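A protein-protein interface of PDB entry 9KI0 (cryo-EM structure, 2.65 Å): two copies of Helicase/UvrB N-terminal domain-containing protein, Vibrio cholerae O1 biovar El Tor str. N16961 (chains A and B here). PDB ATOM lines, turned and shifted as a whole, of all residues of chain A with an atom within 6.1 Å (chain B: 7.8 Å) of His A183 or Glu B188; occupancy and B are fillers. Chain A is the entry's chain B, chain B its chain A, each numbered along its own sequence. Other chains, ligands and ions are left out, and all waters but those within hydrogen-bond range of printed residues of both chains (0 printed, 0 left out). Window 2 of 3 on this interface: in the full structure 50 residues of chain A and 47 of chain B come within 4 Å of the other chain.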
ATOM      1  N   SER A 175      18.373  -1.052  11.018  1.00  0.00           N
ATOM      2  CA  SER A 175      19.015  -1.166  12.322  1.00  0.00           C
ATOM      3  C   SER A 175      19.373   0.211  12.859  1.00  0.00           C
ATOM      4  O   SER A 175      19.189   0.488  14.053  1.00  0.00           O
ATOM      5  CB  SER A 175      20.255  -2.052  12.227  1.00  0.00           C
ATOM      6  OG  SER A 175      20.834  -1.982  10.938  1.00  0.00           O
ATOM      7  N   ALA A 176      19.833   1.106  11.978  1.00  0.00           N
ATOM      8  CA  ALA A 176      20.117   2.470  12.408  1.00  0.00           C
ATOM      9  C   ALA A 176      18.843   3.174  12.860  1.00  0.00           C
ATOM     10  O   ALA A 176      18.850   3.899  13.862  1.00  0.00           O
ATOM     11  CB  ALA A 176      20.792   3.248  11.280  1.00  0.00           C
ATOM     12  N   SER A 178      15.998   1.809  14.066  1.00  0.00           N
ATOM     13  CA  SER A 178      15.534   1.264  15.337  1.00  0.00           C
ATOM     14  C   SER A 178      16.421   1.718  16.490  1.00  0.00           C
ATOM     15  O   SER A 178      15.922   2.065  17.571  1.00  0.00           O
ATOM     16  CB  SER A 178      15.480  -0.262  15.265  1.00  0.00           C
ATOM     17  OG  SER A 178      16.506  -0.768  14.432  1.00  0.00           O
ATOM     18  N   GLY A 179      17.737   1.781  16.262  1.00  0.00           N
ATOM     19  CA  GLY A 179      18.623   2.256  17.307  1.00  0.00           C
ATOM     20  C   GLY A 179      18.385   3.713  17.644  1.00  0.00           C
ATOM     21  O   GLY A 179      18.338   4.086  18.819  1.00  0.00           O
ATOM     22  N   LEU A 180      18.227   4.558  16.624  1.00  0.00           N
ATOM     23  CA  LEU A 180      18.016   5.975  16.888  1.00  0.00           C
ATOM     24  C   LEU A 180      16.678   6.208  17.576  1.00  0.00           C
ATOM     25  O   LEU A 180      16.574   7.049  18.476  1.00  0.00           O
ATOM     26  CB  LEU A 180      18.100   6.774  15.589  1.00  0.00           C
ATOM     27  CG  LEU A 180      18.374   8.268  15.759  1.00  0.00           C
ATOM     28  CD1 LEU A 180      19.584   8.489  16.648  1.00  0.00           C
ATOM     29  CD2 LEU A 180      18.572   8.927  14.411  1.00  0.00           C
ATOM     30  N   ARG A 181      15.640   5.474  17.168  1.00  0.00           N
ATOM     31  CA  ARG A 181      14.320   5.668  17.751  1.00  0.00           C
ATOM     32  C   ARG A 181      14.192   5.048  19.135  1.00  0.00           C
ATOM     33  O   ARG A 181      13.239   5.370  19.851  1.00  0.00           O
ATOM     34  CB  ARG A 181      13.237   5.099  16.833  1.00  0.00           C
ATOM     35  CG  ARG A 181      13.087   3.593  16.892  1.00  0.00           C
ATOM     36  CD  ARG A 181      12.202   3.099  15.762  1.00  0.00           C
ATOM     37  NE  ARG A 181      10.814   3.499  15.951  1.00  0.00           N
ATOM     38  CZ  ARG A 181       9.786   2.982  15.291  1.00  0.00           C
ATOM     39  NH1 ARG A 181       9.955   2.046  14.372  1.00  0.00           N
ATOM     40  NH2 ARG A 181       8.559   3.419  15.557  1.00  0.00           N
ATOM     41  N   ARG A 182      15.114   4.165  19.530  1.00  0.00           N
ATOM     42  CA  ARG A 182      15.046   3.622  20.884  1.00  0.00           C
ATOM     43  C   ARG A 182      15.385   4.685  21.924  1.00  0.00           C
ATOM     44  O   ARG A 182      14.675   4.837  22.925  1.00  0.00           O
ATOM     45  CB  ARG A 182      15.976   2.418  21.017  1.00  0.00           C
ATOM     46  CG  ARG A 182      15.250   1.126  21.357  1.00  0.00           C
ATOM     47  CD  ARG A 182      16.227   0.037  21.786  1.00  0.00           C
ATOM     48  NE  ARG A 182      16.894  -0.615  20.663  1.00  0.00           N
ATOM     49  CZ  ARG A 182      16.280  -1.280  19.691  1.00  0.00           C
ATOM     50  NH1 ARG A 182      14.968  -1.444  19.682  1.00  0.00           N
ATOM     51  NH2 ARG A 182      17.005  -1.806  18.708  1.00  0.00           N
ATOM     52  N   HIS A 183      16.464   5.434  21.704  1.00  0.00           N
ATOM     53  CA  HIS A 183      16.834   6.544  22.586  1.00  0.00           C
ATOM     54  C   HIS A 183      16.247   7.863  22.076  1.00  0.00           C
ATOM     55  O   HIS A 183      16.950   8.845  21.842  1.00  0.00           O
ATOM     56  CB  HIS A 183      18.350   6.628  22.733  1.00  0.00           C
ATOM     57  CG  HIS A 183      19.048   5.310  22.603  1.00  0.00           C
ATOM     58  ND1 HIS A 183      19.407   4.547  23.693  1.00  0.00           N
ATOM     59  CD2 HIS A 183      19.467   4.625  21.513  1.00  0.00           C
ATOM     60  CE1 HIS A 183      20.007   3.445  23.281  1.00  0.00           C
ATOM     61  NE2 HIS A 183      20.057   3.469  21.961  1.00  0.00           N
ATOM     62  N   ALA A 184      14.928   7.872  21.908  1.00  0.00           N
ATOM     63  CA  ALA A 184      14.226   9.016  21.343  1.00  0.00           C
ATOM     64  C   ALA A 184      13.735  10.002  22.399  1.00  0.00           C
ATOM     65  O   ALA A 184      13.022  10.951  22.056  1.00  0.00           O
ATOM     66  CB  ALA A 184      13.045   8.542  20.495  1.00  0.00           C
ATOM     67  N   SER A 185      14.094   9.801  23.670  1.00  0.00           N
ATOM     68  CA  SER A 185      13.648  10.713  24.720  1.00  0.00           C
ATOM     69  C   SER A 185      14.206  12.115  24.512  1.00  0.00           C
ATOM     70  O   SER A 185      13.501  13.110  24.722  1.00  0.00           O
ATOM     71  CB  SER A 185      14.056  10.172  26.090  1.00  0.00           C
ATOM     72  OG  SER A 185      13.917  11.164  27.092  1.00  0.00           O
ATOM     73  N   ASN A 186      15.468  12.213  24.112  1.00  0.00           N
ATOM     74  CA  ASN A 186      16.079  13.514  23.886  1.00  0.00           C
ATOM     75  C   ASN A 186      15.378  14.226  22.730  1.00  0.00           C
ATOM     76  O   ASN A 186      14.990  13.582  21.749  1.00  0.00           O
ATOM     77  CB  ASN A 186      17.568  13.349  23.585  1.00  0.00           C
ATOM     78  CG  ASN A 186      18.175  12.151  24.281  1.00  0.00           C
ATOM     79  OD1 ASN A 186      18.131  11.034  23.769  1.00  0.00           O
ATOM     80  ND2 ASN A 186      18.753  12.378  25.454  1.00  0.00           N
ATOM     81  N   VAL A 189      17.331  14.217  19.122  1.00  0.00           N
ATOM     82  CA  VAL A 189      17.300  12.963  18.382  1.00  0.00           C
ATOM     83  C   VAL A 189      16.083  12.916  17.468  1.00  0.00           C
ATOM     84  O   VAL A 189      16.148  12.358  16.365  1.00  0.00           O
ATOM     85  CB  VAL A 189      17.330  11.772  19.360  1.00  0.00           C
ATOM     86  CG1 VAL A 189      16.806  10.509  18.702  1.00  0.00           C
ATOM     87  CG2 VAL A 189      18.741  11.544  19.871  1.00  0.00           C
ATOM     88  N   LEU B 180      23.179  15.231  17.141  1.00  0.00           N
ATOM     89  CA  LEU B 180      23.523  13.830  17.299  1.00  0.00           C
ATOM     90  C   LEU B 180      24.905  13.712  17.909  1.00  0.00           C
ATOM     91  O   LEU B 180      25.200  12.731  18.600  1.00  0.00           O
ATOM     92  CB  LEU B 180      23.449  13.109  15.953  1.00  0.00           C
ATOM     93  CG  LEU B 180      22.325  12.081  15.802  1.00  0.00           C
ATOM     94  CD1 LEU B 180      22.561  11.196  14.593  1.00  0.00           C
ATOM     95  CD2 LEU B 180      22.167  11.249  17.060  1.00  0.00           C
ATOM     96  N   HIS B 183      24.861  14.039  22.097  1.00  0.00           N
ATOM     97  CA  HIS B 183      24.297  12.908  22.832  1.00  0.00           C
ATOM     98  C   HIS B 183      24.703  11.564  22.242  1.00  0.00           C
ATOM     99  O   HIS B 183      23.877  10.652  22.144  1.00  0.00           O
ATOM    100  CB  HIS B 183      22.780  13.039  22.915  1.00  0.00           C
ATOM    101  CG  HIS B 183      22.304  14.453  23.048  1.00  0.00           C
ATOM    102  ND1 HIS B 183      21.760  14.942  24.216  1.00  0.00           N
ATOM    103  CD2 HIS B 183      22.330  15.495  22.183  1.00  0.00           C
ATOM    104  CE1 HIS B 183      21.444  16.215  24.056  1.00  0.00           C
ATOM    105  NE2 HIS B 183      21.780  16.575  22.831  1.00  0.00           N
ATOM    106  N   SER B 185      25.321   8.170  22.086  1.00  0.00           N
ATOM    107  CA  SER B 185      25.066   7.025  22.949  1.00  0.00           C
ATOM    108  C   SER B 185      25.753   5.790  22.363  1.00  0.00           C
ATOM    109  O   SER B 185      26.653   5.902  21.526  1.00  0.00           O
ATOM    110  CB  SER B 185      23.558   6.834  23.130  1.00  0.00           C
ATOM    111  OG  SER B 185      22.984   7.926  23.827  1.00  0.00           O
ATOM    112  N   ASN B 186      25.348   4.602  22.817  1.00  0.00           N
ATOM    113  CA  ASN B 186      25.809   3.303  22.334  1.00  0.00           C
ATOM    114  C   ASN B 186      25.776   3.237  20.808  1.00  0.00           C
ATOM    115  O   ASN B 186      25.059   4.023  20.174  1.00  0.00           O
ATOM    116  CB  ASN B 186      24.939   2.196  22.938  1.00  0.00           C
ATOM    117  CG  ASN B 186      25.191   2.000  24.422  1.00  0.00           C
ATOM    118  OD1 ASN B 186      26.254   2.349  24.936  1.00  0.00           O
ATOM    119  ND2 ASN B 186      24.209   1.438  25.119  1.00  0.00           N
ATOM    120  N   PRO B 187      26.534   2.306  20.176  1.00  0.00           N
ATOM    121  CA  PRO B 187      26.676   2.312  18.707  1.00  0.00           C
ATOM    122  C   PRO B 187      25.383   2.427  17.910  1.00  0.00           C
ATOM    123  O   PRO B 187      25.422   2.743  16.713  1.00  0.00           O
ATOM    124  CB  PRO B 187      27.368   0.968  18.418  1.00  0.00           C
ATOM    125  CG  PRO B 187      27.452   0.239  19.741  1.00  0.00           C
ATOM    126  CD  PRO B 187      27.396   1.287  20.793  1.00  0.00           C
ATOM    127  N   GLU B 188      24.238   2.198  18.561  1.00  0.00           N
ATOM    128  CA  GLU B 188      22.952   2.358  17.888  1.00  0.00           C
ATOM    129  C   GLU B 188      22.822   3.763  17.315  1.00  0.00           C
ATOM    130  O   GLU B 188      22.397   3.945  16.169  1.00  0.00           O
ATOM    131  CB  GLU B 188      21.813   2.065  18.866  1.00  0.00           C
ATOM    132  CG  GLU B 188      21.749   0.626  19.356  1.00  0.00           C
ATOM    133  CD  GLU B 188      20.891  -0.257  18.472  1.00  0.00           C
ATOM    134  OE1 GLU B 188      21.107  -0.268  17.241  1.00  0.00           O
ATOM    135  OE2 GLU B 188      19.992  -0.940  19.007  1.00  0.00           O
ATOM    136  N   VAL B 189      23.183   4.770  18.111  1.00  0.00           N
ATOM    137  CA  VAL B 189      23.222   6.141  17.620  1.00  0.00           C
ATOM    138  C   VAL B 189      24.355   6.310  16.613  1.00  0.00           C
ATOM    139  O   VAL B 189      24.225   7.047  15.628  1.00  0.00           O
ATOM    140  CB  VAL B 189      23.352   7.117  18.804  1.00  0.00           C
ATOM    141  CG1 VAL B 189      24.036   8.408  18.382  1.00  0.00           C
ATOM    142  CG2 VAL B 189      21.985   7.406  19.401  1.00  0.00           C
ATOM    143  N   LYS B 190      25.481   5.628  16.845  1.00  0.00           N
ATOM    144  CA  LYS B 190      26.705   5.899  16.099  1.00  0.00           C
ATOM    145  C   LYS B 190      26.605   5.506  14.627  1.00  0.00           C
ATOM    146  O   LYS B 190      27.183   6.190  13.774  1.00  0.00           O
ATOM    147  CB  LYS B 190      27.878   5.173  16.758  1.00  0.00           C
ATOM    148  CG  LYS B 190      28.761   6.067  17.614  1.00  0.00           C
ATOM    149  CD  LYS B 190      29.592   7.007  16.761  1.00  0.00           C
ATOM    150  CE  LYS B 190      30.569   6.236  15.888  1.00  0.00           C
ATOM    151  NZ  LYS B 190      31.135   7.086  14.805  1.00  0.00           N
ATOM    152  N   ILE B 191      25.886   4.426  14.299  1.00  0.00           N
ATOM    153  CA  ILE B 191      25.703   4.090  12.884  1.00  0.00           C
ATOM    154  C   ILE B 191      24.968   5.210  12.156  1.00  0.00           C
ATOM    155  O   ILE B 191      25.361   5.630  11.053  1.00  0.00           O
ATOM    156  CB  ILE B 191      24.966   2.746  12.732  1.00  0.00           C
ATOM    157  CG1 ILE B 191      25.357   1.774  13.844  1.00  0.00           C
ATOM    158  CG2 ILE B 191      25.233   2.140  11.362  1.00  0.00           C
ATOM    159  CD1 ILE B 191      26.732   1.167  13.676  1.00  0.00           C
ATOM    160  N   SER B 192      23.924   5.750  12.786  1.00  0.00           N
ATOM    161  CA  SER B 192      23.178   6.840  12.174  1.00  0.00           C
ATOM    162  C   SER B 192      24.041   8.086  12.081  1.00  0.00           C
ATOM    163  O   SER B 192      23.995   8.808  11.078  1.00  0.00           O
ATOM    164  CB  SER B 192      21.905   7.117  12.971  1.00  0.00           C
ATOM    165  OG  SER B 192      22.203   7.395  14.326  1.00  0.00           O
ATOM    166  N   LEU B 193      24.845   8.342  13.112  1.00  0.00           N
ATOM    167  CA  LEU B 193      25.683   9.533  13.099  1.00  0.00           C
ATOM    168  C   LEU B 193      26.691   9.454  11.965  1.00  0.00           C
ATOM    169  O   LEU B 193      26.941  10.450  11.282  1.00  0.00           O
ATOM    170  CB  LEU B 193      26.389   9.698  14.442  1.00  0.00           C
ATOM    171  CG  LEU B 193      27.292  10.923  14.585  1.00  0.00           C
ATOM    172  CD1 LEU B 193      26.571  12.177  14.127  1.00  0.00           C
ATOM    173  CD2 LEU B 193      27.772  11.074  16.016  1.00  0.00           C
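Printed residues of chain B within 4 Å of Ser A175: Glu B188.
Of the printed residues of chain B, His A183 touches Glu B188 (3.8 Å).
Ala A184 touches none of the printed residues of chain B.
Printed residues of chain A within 4 Å of Leu B180: Leu A180.
Of the printed residues of chain A, Glu B188 touches Ser A175, Gly A179, Arg A182 and His A183.
Of the printed residues of chain A, Ser B192 touches Leu A180.
The nearest printed residue of chain A that does not touch Ser B192 is Ala A176 (4.3 Å).
The guanidinium group of Arg A182 is in salt-bridge range of the side-chain carboxylate of Glu B188 (3.1 Å).
The backbone carbonyl oxygen of His A183 lies close to the side-chain amide oxygen of Asn A186 (3.1 Å).
O of Ser A175 lies within hydrogen-bond range of OG of Ser A178 (3.0 Å).
The side-chain hydroxyl (OG) of Ser B192 is in hydrogen-bond range of the backbone carbonyl oxygen (O) of Val B189 (2.4 Å).
Leu B180 touches its own counterpart, Leu A180.
Leu A180 touches Val B189, but with the chains exchanged Val A189 does not touch Leu B180 (4.4 Å).
Of the 7 pairs that touch across the chains among the printed residues, 1 has its exchanged pair printed and touching as well.
Hydrophobic or aromatic side chains of chain B within 4 Å of the printed part of chain A: Leu B180 and Val B189.
Along chain B the printed residues that touch a printed residue of chain A span positions 180 to 192.
Of the 12 printed residues of chain A, 5 touch a printed residue of chain B.
Among the printed residues, 7 pairs touch across the chains.
Among the printed residues, pairs that only touch across the chains: Ser A175 with Glu B188 (3.8 Å), Gly A179 with Glu B188 (3.5 Å), Leu A180 with Leu B180 (3.8 Å), Leu A180 with Val B189 (3.8 Å), Leu A180 with Ser B192 (3.7 Å) and His A183 with Glu B188 (3.8 Å).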
